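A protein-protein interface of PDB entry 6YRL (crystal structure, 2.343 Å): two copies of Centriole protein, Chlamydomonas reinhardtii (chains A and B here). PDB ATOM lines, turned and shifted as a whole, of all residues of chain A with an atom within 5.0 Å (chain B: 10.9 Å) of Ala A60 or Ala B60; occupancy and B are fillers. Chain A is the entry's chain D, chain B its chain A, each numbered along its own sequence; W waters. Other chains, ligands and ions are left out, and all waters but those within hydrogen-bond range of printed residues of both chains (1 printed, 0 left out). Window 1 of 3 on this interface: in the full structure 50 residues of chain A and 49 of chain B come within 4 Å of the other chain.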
ATOM      1  N   GLN A  56     -23.779  22.607  -5.649  1.00  0.00           N
ATOM      2  CA  GLN A  56     -24.816  21.615  -5.366  1.00  0.00           C
ATOM      3  C   GLN A  56     -25.282  21.686  -3.914  1.00  0.00           C
ATOM      4  O   GLN A  56     -26.487  21.620  -3.636  1.00  0.00           O
ATOM      5  CB  GLN A  56     -24.297  20.221  -5.693  1.00  0.00           C
ATOM      6  CG  GLN A  56     -24.106  20.009  -7.175  1.00  0.00           C
ATOM      7  CD  GLN A  56     -23.672  18.605  -7.517  1.00  0.00           C
ATOM      8  OE1 GLN A  56     -24.004  17.647  -6.814  1.00  0.00           O
ATOM      9  NE2 GLN A  56     -22.917  18.473  -8.604  1.00  0.00           N
ATOM     10  N   LEU A  57     -24.344  21.830  -2.978  1.00  0.00           N
ATOM     11  CA  LEU A  57     -24.705  21.940  -1.569  1.00  0.00           C
ATOM     12  C   LEU A  57     -25.605  23.143  -1.325  1.00  0.00           C
ATOM     13  O   LEU A  57     -26.599  23.041  -0.596  1.00  0.00           O
ATOM     14  CB  LEU A  57     -23.443  22.030  -0.709  1.00  0.00           C
ATOM     15  CG  LEU A  57     -23.666  22.174   0.797  1.00  0.00           C
ATOM     16  CD1 LEU A  57     -24.343  20.929   1.359  1.00  0.00           C
ATOM     17  CD2 LEU A  57     -22.341  22.420   1.502  1.00  0.00           C
ATOM     18  N   ASN A  58     -25.285  24.285  -1.939  1.00  0.00           N
ATOM     19  CA  ASN A  58     -26.124  25.472  -1.789  1.00  0.00           C
ATOM     20  C   ASN A  58     -27.538  25.209  -2.285  1.00  0.00           C
ATOM     21  O   ASN A  58     -28.522  25.523  -1.598  1.00  0.00           O
ATOM     22  CB  ASN A  58     -25.508  26.655  -2.538  1.00  0.00           C
ATOM     23  CG  ASN A  58     -24.450  27.377  -1.728  1.00  0.00           C
ATOM     24  OD1 ASN A  58     -24.357  27.208  -0.508  1.00  0.00           O
ATOM     25  ND2 ASN A  58     -23.647  28.192  -2.403  1.00  0.00           N
ATOM     26  N   GLU A  59     -27.664  24.621  -3.481  1.00  0.00           N
ATOM     27  CA  GLU A  59     -28.998  24.326  -3.993  1.00  0.00           C
ATOM     28  C   GLU A  59     -29.754  23.386  -3.053  1.00  0.00           C
ATOM     29  O   GLU A  59     -30.919  23.640  -2.715  1.00  0.00           O
ATOM     30  CB  GLU A  59     -28.895  23.752  -5.411  1.00  0.00           C
ATOM     31  CG  GLU A  59     -28.095  24.668  -6.355  1.00  0.00           C
ATOM     32  CD  GLU A  59     -28.119  24.236  -7.822  1.00  0.00           C
ATOM     33  OE1 GLU A  59     -28.337  23.033  -8.092  1.00  0.00           O
ATOM     34  OE2 GLU A  59     -27.903  25.106  -8.704  1.00  0.00           O
ATOM     35  N   ALA A  60     -29.094  22.325  -2.568  1.00  0.00           N
ATOM     36  CA  ALA A  60     -29.775  21.387  -1.673  1.00  0.00           C
ATOM     37  C   ALA A  60     -30.203  22.057  -0.369  1.00  0.00           C
ATOM     38  O   ALA A  60     -31.317  21.829   0.115  1.00  0.00           O
ATOM     39  CB  ALA A  60     -28.878  20.182  -1.383  1.00  0.00           C
ATOM     40  N   LYS A  61     -29.330  22.878   0.218  1.00  0.00           N
ATOM     41  CA  LYS A  61     -29.715  23.620   1.415  1.00  0.00           C
ATOM     42  C   LYS A  61     -30.968  24.447   1.167  1.00  0.00           C
ATOM     43  O   LYS A  61     -31.934  24.371   1.939  1.00  0.00           O
ATOM     44  CB  LYS A  61     -28.562  24.513   1.878  1.00  0.00           C
ATOM     45  CG  LYS A  61     -27.457  23.773   2.639  1.00  0.00           C
ATOM     46  CD  LYS A  61     -26.586  24.738   3.427  1.00  0.00           C
ATOM     47  CE  LYS A  61     -25.150  24.250   3.497  1.00  0.00           C
ATOM     48  NZ  LYS A  61     -24.197  25.390   3.660  1.00  0.00           N
ATOM     49  N   ALA A  62     -30.980  25.230   0.080  1.00  0.00           N
ATOM     50  CA  ALA A  62     -32.174  26.014  -0.236  1.00  0.00           C
ATOM     51  C   ALA A  62     -33.408  25.125  -0.321  1.00  0.00           C
ATOM     52  O   ALA A  62     -34.460  25.453   0.247  1.00  0.00           O
ATOM     53  CB  ALA A  62     -31.974  26.786  -1.541  1.00  0.00           C
ATOM     54  N   LYS A  63     -33.296  23.979  -1.004  1.00  0.00           N
ATOM     55  CA  LYS A  63     -34.439  23.073  -1.083  1.00  0.00           C
ATOM     56  C   LYS A  63     -34.888  22.628   0.302  1.00  0.00           C
ATOM     57  O   LYS A  63     -36.093  22.512   0.563  1.00  0.00           O
ATOM     58  CB  LYS A  63     -34.114  21.857  -1.946  1.00  0.00           C
ATOM     59  CG  LYS A  63     -35.369  21.209  -2.520  1.00  0.00           C
ATOM     60  CD  LYS A  63     -35.069  20.434  -3.787  1.00  0.00           C
ATOM     61  CE  LYS A  63     -36.216  19.480  -4.116  1.00  0.00           C
ATOM     62  NZ  LYS A  63     -36.004  18.737  -5.408  1.00  0.00           N
ATOM     63  N   VAL A  64     -33.941  22.391   1.214  1.00  0.00           N
ATOM     64  CA  VAL A  64     -34.339  22.021   2.567  1.00  0.00           C
ATOM     65  C   VAL A  64     -35.113  23.161   3.225  1.00  0.00           C
ATOM     66  O   VAL A  64     -36.167  22.939   3.828  1.00  0.00           O
ATOM     67  CB  VAL A  64     -33.125  21.598   3.411  1.00  0.00           C
ATOM     68  CG1 VAL A  64     -33.551  21.389   4.852  1.00  0.00           C
ATOM     69  CG2 VAL A  64     -32.512  20.325   2.866  1.00  0.00           C
ATOM     70  N   GLU B  52     -15.468  16.752   3.022  1.00  0.00           N
ATOM     71  CA  GLU B  52     -16.409  17.411   3.922  1.00  0.00           C
ATOM     72  C   GLU B  52     -17.664  17.851   3.179  1.00  0.00           C
ATOM     73  O   GLU B  52     -18.796  17.584   3.618  1.00  0.00           O
ATOM     74  CB  GLU B  52     -15.728  18.603   4.594  1.00  0.00           C
ATOM     75  CG  GLU B  52     -16.645  19.448   5.460  1.00  0.00           C
ATOM     76  CD  GLU B  52     -17.333  18.640   6.537  1.00  0.00           C
ATOM     77  OE1 GLU B  52     -16.751  17.625   6.982  1.00  0.00           O
ATOM     78  OE2 GLU B  52     -18.450  19.022   6.958  1.00  0.00           O
ATOM     79  N   LEU B  53     -17.482  18.521   2.037  1.00  0.00           N
ATOM     80  CA  LEU B  53     -18.626  18.947   1.238  1.00  0.00           C
ATOM     81  C   LEU B  53     -19.454  17.756   0.779  1.00  0.00           C
ATOM     82  O   LEU B  53     -20.686  17.846   0.725  1.00  0.00           O
ATOM     83  CB  LEU B  53     -18.154  19.758   0.036  1.00  0.00           C
ATOM     84  CG  LEU B  53     -17.600  21.146   0.348  1.00  0.00           C
ATOM     85  CD1 LEU B  53     -16.887  21.719  -0.863  1.00  0.00           C
ATOM     86  CD2 LEU B  53     -18.717  22.061   0.794  1.00  0.00           C
ATOM     87  N   GLU B  54     -18.802  16.630   0.470  1.00  0.00           N
ATOM     88  CA  GLU B  54     -19.528  15.413   0.115  1.00  0.00           C
ATOM     89  C   GLU B  54     -20.433  14.963   1.251  1.00  0.00           C
ATOM     90  O   GLU B  54     -21.625  14.700   1.046  1.00  0.00           O
ATOM     91  CB  GLU B  54     -18.541  14.304  -0.256  1.00  0.00           C
ATOM     92  CG  GLU B  54     -18.177  14.296  -1.734  1.00  0.00           C
ATOM     93  CD  GLU B  54     -16.880  13.559  -2.030  1.00  0.00           C
ATOM     94  OE1 GLU B  54     -16.344  12.875  -1.125  1.00  0.00           O
ATOM     95  OE2 GLU B  54     -16.399  13.669  -3.179  1.00  0.00           O
ATOM     96  N   ILE B  55     -19.886  14.875   2.466  1.00  0.00           N
ATOM     97  CA  ILE B  55     -20.696  14.458   3.607  1.00  0.00           C
ATOM     98  C   ILE B  55     -21.895  15.387   3.776  1.00  0.00           C
ATOM     99  O   ILE B  55     -23.045  14.936   3.913  1.00  0.00           O
ATOM    100  CB  ILE B  55     -19.828  14.388   4.880  1.00  0.00           C
ATOM    101  CG1 ILE B  55     -18.810  13.250   4.748  1.00  0.00           C
ATOM    102  CG2 ILE B  55     -20.683  14.164   6.114  1.00  0.00           C
ATOM    103  CD1 ILE B  55     -17.857  13.133   5.909  1.00  0.00           C
ATOM    104  N   GLN B  56     -21.654  16.701   3.716  1.00  0.00           N
ATOM    105  CA  GLN B  56     -22.749  17.648   3.931  1.00  0.00           C
ATOM    106  C   GLN B  56     -23.805  17.546   2.830  1.00  0.00           C
ATOM    107  O   GLN B  56     -25.010  17.625   3.105  1.00  0.00           O
ATOM    108  CB  GLN B  56     -22.192  19.069   4.023  1.00  0.00           C
ATOM    109  CG  GLN B  56     -21.616  19.407   5.391  1.00  0.00           C
ATOM    110  CD  GLN B  56     -21.222  20.877   5.525  1.00  0.00           C
ATOM    111  OE1 GLN B  56     -22.010  21.784   5.233  1.00  0.00           O
ATOM    112  NE2 GLN B  56     -19.991  21.113   5.968  1.00  0.00           N
ATOM    113  N   LEU B  57     -23.379  17.363   1.575  1.00  0.00           N
ATOM    114  CA  LEU B  57     -24.350  17.225   0.492  1.00  0.00           C
ATOM    115  C   LEU B  57     -25.191  15.965   0.661  1.00  0.00           C
ATOM    116  O   LEU B  57     -26.413  16.002   0.480  1.00  0.00           O
ATOM    117  CB  LEU B  57     -23.638  17.208  -0.859  1.00  0.00           C
ATOM    118  CG  LEU B  57     -24.509  16.938  -2.087  1.00  0.00           C
ATOM    119  CD1 LEU B  57     -25.482  18.093  -2.337  1.00  0.00           C
ATOM    120  CD2 LEU B  57     -23.623  16.717  -3.303  1.00  0.00           C
ATOM    121  N   ASN B  58     -24.555  14.839   1.001  1.00  0.00           N
ATOM    122  CA  ASN B  58     -25.317  13.619   1.254  1.00  0.00           C
ATOM    123  C   ASN B  58     -26.358  13.842   2.347  1.00  0.00           C
ATOM    124  O   ASN B  58     -27.539  13.503   2.177  1.00  0.00           O
ATOM    125  CB  ASN B  58     -24.370  12.475   1.621  1.00  0.00           C
ATOM    126  CG  ASN B  58     -23.590  11.965   0.419  1.00  0.00           C
ATOM    127  OD1 ASN B  58     -23.923  12.282  -0.724  1.00  0.00           O
ATOM    128  ND2 ASN B  58     -22.543  11.182   0.670  1.00  0.00           N
ATOM    129  N   GLU B  59     -25.942  14.447   3.465  1.00  0.00           N
ATOM    130  CA  GLU B  59     -26.888  14.754   4.536  1.00  0.00           C
ATOM    131  C   GLU B  59     -28.054  15.592   4.018  1.00  0.00           C
ATOM    132  O   GLU B  59     -29.226  15.265   4.255  1.00  0.00           O
ATOM    133  CB  GLU B  59     -26.169  15.480   5.673  1.00  0.00           C
ATOM    134  CG  GLU B  59     -25.706  14.585   6.806  1.00  0.00           C
ATOM    135  CD  GLU B  59     -24.811  15.315   7.794  1.00  0.00           C
ATOM    136  OE1 GLU B  59     -23.874  14.676   8.330  1.00  0.00           O
ATOM    137  OE2 GLU B  59     -25.041  16.524   8.026  1.00  0.00           O
ATOM    138  N   ALA B  60     -27.746  16.676   3.297  1.00  0.00           N
ATOM    139  CA  ALA B  60     -28.789  17.585   2.829  1.00  0.00           C
ATOM    140  C   ALA B  60     -29.771  16.881   1.899  1.00  0.00           C
ATOM    141  O   ALA B  60     -30.989  17.028   2.043  1.00  0.00           O
ATOM    142  CB  ALA B  60     -28.156  18.787   2.132  1.00  0.00           C
ATOM    143  N   LYS B  61     -29.259  16.115   0.930  1.00  0.00           N
ATOM    144  CA  LYS B  61     -30.148  15.369   0.038  1.00  0.00           C
ATOM    145  C   LYS B  61     -31.044  14.412   0.820  1.00  0.00           C
ATOM    146  O   LYS B  61     -32.240  14.275   0.516  1.00  0.00           O
ATOM    147  CB  LYS B  61     -29.329  14.612  -1.007  1.00  0.00           C
ATOM    148  CG  LYS B  61     -28.672  15.526  -2.037  1.00  0.00           C
ATOM    149  CD  LYS B  61     -28.646  14.885  -3.421  1.00  0.00           C
ATOM    150  CE  LYS B  61     -27.603  15.540  -4.317  1.00  0.00           C
ATOM    151  NZ  LYS B  61     -28.024  15.608  -5.747  1.00  0.00           N
ATOM    152  N   ALA B  62     -30.493  13.756   1.845  1.00  0.00           N
ATOM    153  CA  ALA B  62     -31.326  12.886   2.670  1.00  0.00           C
ATOM    154  C   ALA B  62     -32.445  13.681   3.321  1.00  0.00           C
ATOM    155  O   ALA B  62     -33.626  13.312   3.222  1.00  0.00           O
ATOM    156  CB  ALA B  62     -30.483  12.175   3.728  1.00  0.00           C
ATOM    157  N   LYS B  63     -32.095  14.798   3.970  1.00  0.00           N
ATOM    158  CA  LYS B  63     -33.124  15.642   4.568  1.00  0.00           C
ATOM    159  C   LYS B  63     -34.171  16.054   3.541  1.00  0.00           C
ATOM    160  O   LYS B  63     -35.362  16.101   3.867  1.00  0.00           O
ATOM    161  CB  LYS B  63     -32.497  16.873   5.225  1.00  0.00           C
ATOM    162  CG  LYS B  63     -33.201  17.275   6.516  1.00  0.00           C
ATOM    163  CD  LYS B  63     -32.831  18.674   6.997  1.00  0.00           C
ATOM    164  CE  LYS B  63     -33.744  19.115   8.143  1.00  0.00           C
ATOM    165  NZ  LYS B  63     -33.261  20.351   8.816  1.00  0.00           N
ATOM    166  N   VAL B  64     -33.764  16.319   2.295  1.00  0.00           N
ATOM    167  CA  VAL B  64     -34.741  16.645   1.254  1.00  0.00           C
ATOM    168  C   VAL B  64     -35.727  15.502   1.067  1.00  0.00           C
ATOM    169  O   VAL B  64     -36.941  15.723   0.959  1.00  0.00           O
ATOM    170  CB  VAL B  64     -34.043  16.984  -0.074  1.00  0.00           C
ATOM    171  CG1 VAL B  64     -35.091  17.074  -1.201  1.00  0.00           C
ATOM    172  CG2 VAL B  64     -33.270  18.283   0.058  1.00  0.00           C
ATOM    173  N   LEU B  65     -35.224  14.264   1.003  1.00  0.00           N
ATOM    174  CA  LEU B  65     -36.123  13.121   0.861  1.00  0.00           C
ATOM    175  C   LEU B  65     -37.102  13.041   2.029  1.00  0.00           C
ATOM    176  O   LEU B  65     -38.322  12.998   1.830  1.00  0.00           O
ATOM    177  CB  LEU B  65     -35.316  11.831   0.747  1.00  0.00           C
ATOM    178  CG  LEU B  65     -34.722  11.568  -0.636  1.00  0.00           C
ATOM    179  CD1 LEU B  65     -34.091  10.181  -0.692  1.00  0.00           C
ATOM    180  CD2 LEU B  65     -35.775  11.744  -1.728  1.00  0.00           C
ATOM    181  N   ALA B  66     -36.581  13.035   3.262  1.00  0.00           N
ATOM    182  CA  ALA B  66     -37.441  12.951   4.442  1.00  0.00           C
ATOM    183  C   ALA B  66     -38.500  14.053   4.449  1.00  0.00           C
ATOM    184  O   ALA B  66     -39.704  13.784   4.589  1.00  0.00           O
ATOM    185  CB  ALA B  66     -36.586  13.021   5.708  1.00  0.00           C
ATOM    186  N   LEU B  67     -38.068  15.306   4.294  1.00  0.00           N
ATOM    187  CA  LEU B  67     -39.016  16.416   4.320  1.00  0.00           C
ATOM    188  C   LEU B  67     -40.015  16.339   3.172  1.00  0.00           C
ATOM    189  O   LEU B  67     -41.184  16.694   3.352  1.00  0.00           O
ATOM    190  CB  LEU B  67     -38.264  17.743   4.289  1.00  0.00           C
ATOM    191  CG  LEU B  67     -37.594  18.073   5.625  1.00  0.00           C
ATOM    192  CD1 LEU B  67     -36.552  19.156   5.428  1.00  0.00           C
ATOM    193  CD2 LEU B  67     -38.623  18.488   6.685  1.00  0.00           C
ATOM    194  N   ASP B  68     -39.591  15.882   1.992  1.00  0.00           N
ATOM    195  CA  ASP B  68     -40.543  15.738   0.891  1.00  0.00           C
ATOM    196  C   ASP B  68     -41.593  14.682   1.219  1.00  0.00           C
ATOM    197  O   ASP B  68     -42.788  14.886   0.973  1.00  0.00           O
ATOM    198  CB  ASP B  68     -39.809  15.388  -0.406  1.00  0.00           C
ATOM    199  CG  ASP B  68     -40.712  15.467  -1.633  1.00  0.00           C
ATOM    200  OD1 ASP B  68     -41.213  16.569  -1.944  1.00  0.00           O
ATOM    201  OD2 ASP B  68     -40.921  14.423  -2.289  1.00  0.00           O
ATOM    202  N   GLU B  69     -41.166  13.554   1.793  1.00  0.00           N
ATOM    203  CA  GLU B  69     -42.116  12.547   2.247  1.00  0.00           C
ATOM    204  C   GLU B  69     -43.127  13.158   3.207  1.00  0.00           C
ATOM    205  O   GLU B  69     -44.349  13.074   2.988  1.00  0.00           O
ATOM    206  CB  GLU B  69     -41.364  11.390   2.913  1.00  0.00           C
ATOM    207  CG  GLU B  69     -42.246  10.225   3.355  1.00  0.00           C
ATOM    208  CD  GLU B  69     -41.572   9.332   4.386  1.00  0.00           C
ATOM    209  OE1 GLU B  69     -40.318   9.322   4.446  1.00  0.00           O
ATOM    210  OE2 GLU B  69     -42.295   8.626   5.127  1.00  0.00           O
HETATM  211  O   HOH W   1     -21.522  24.600   4.743  1.00  0.00           O
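The side-chain carboxylate (OE2) of Glu B52 lies within hydrogen-bond range of the side-chain amide nitrogen (NE2) of Gln B56, 2.8 Å away.
Gln A56 touches Leu B57, and with the chains exchanged Leu A57 touches Gln B56.
Lys A63 touches Val B64, and with the chains exchanged Val A64 touches Lys B63.
Val A64 touches Ala B60, but with the chains exchanged Ala A60 does not touch Val B64 (4.05 Å).
Val B64 touches its own counterpart, Val A64.
9 positions are printed for both chains.
Of the 10 pairs that touch across the chains among the printed residues, 7 have their exchanged pair printed and touching as well.
Of the printed residues of chain B, Leu A57 touches Leu B53 (3.7 Å), Gln B56 (3.7 Å) and Leu B57 (3.7 Å).
No residue of chain B comes within 4 Å of Glu A59.
Ala A60 touches just one residue of chain B: Ala B60.
No residue of chain B comes within 4 Å of Ala A62.
Ile B55 touches none of the printed residues of chain A.
Printed residues of chain A within 4 Å of Gln B56: Leu A57 (3.7 Å).
Of the printed residues of chain A, Ala B60 touches Ala A60 (3.9 Å) and Val A64 (3.7 Å).
Of the printed residues of chain A, Leu B67 touches Val A64.
The nearest residue of chain A that does not touch Ala B60 is Leu A57 (4.4 Å).
Among the printed residues, pairs that only touch across the chains: Val A64 with Lys B63, Val A64 with Val B64, Gln A56 with Leu B57, Leu A57 with Leu B57, Leu A57 with Leu B53, Val A64 with Ala B60, Leu A57 with Gln B56, Val A64 with Leu B67, Ala A60 with Ala B60 and Lys A63 with Val B64.
Water W1 bridges OE1 of Gln B56 (2.9 Å) and NZ of Lys A61 (3.0 Å).
Of the 18 printed residues of chain B, 7 touch a printed residue of chain A.
Hydrophobic or aromatic side chains of chain A that line the printed part of chain B: Leu A57, Ala A60 and Val A64.
Among the printed residues, 10 pairs touch across the chains.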
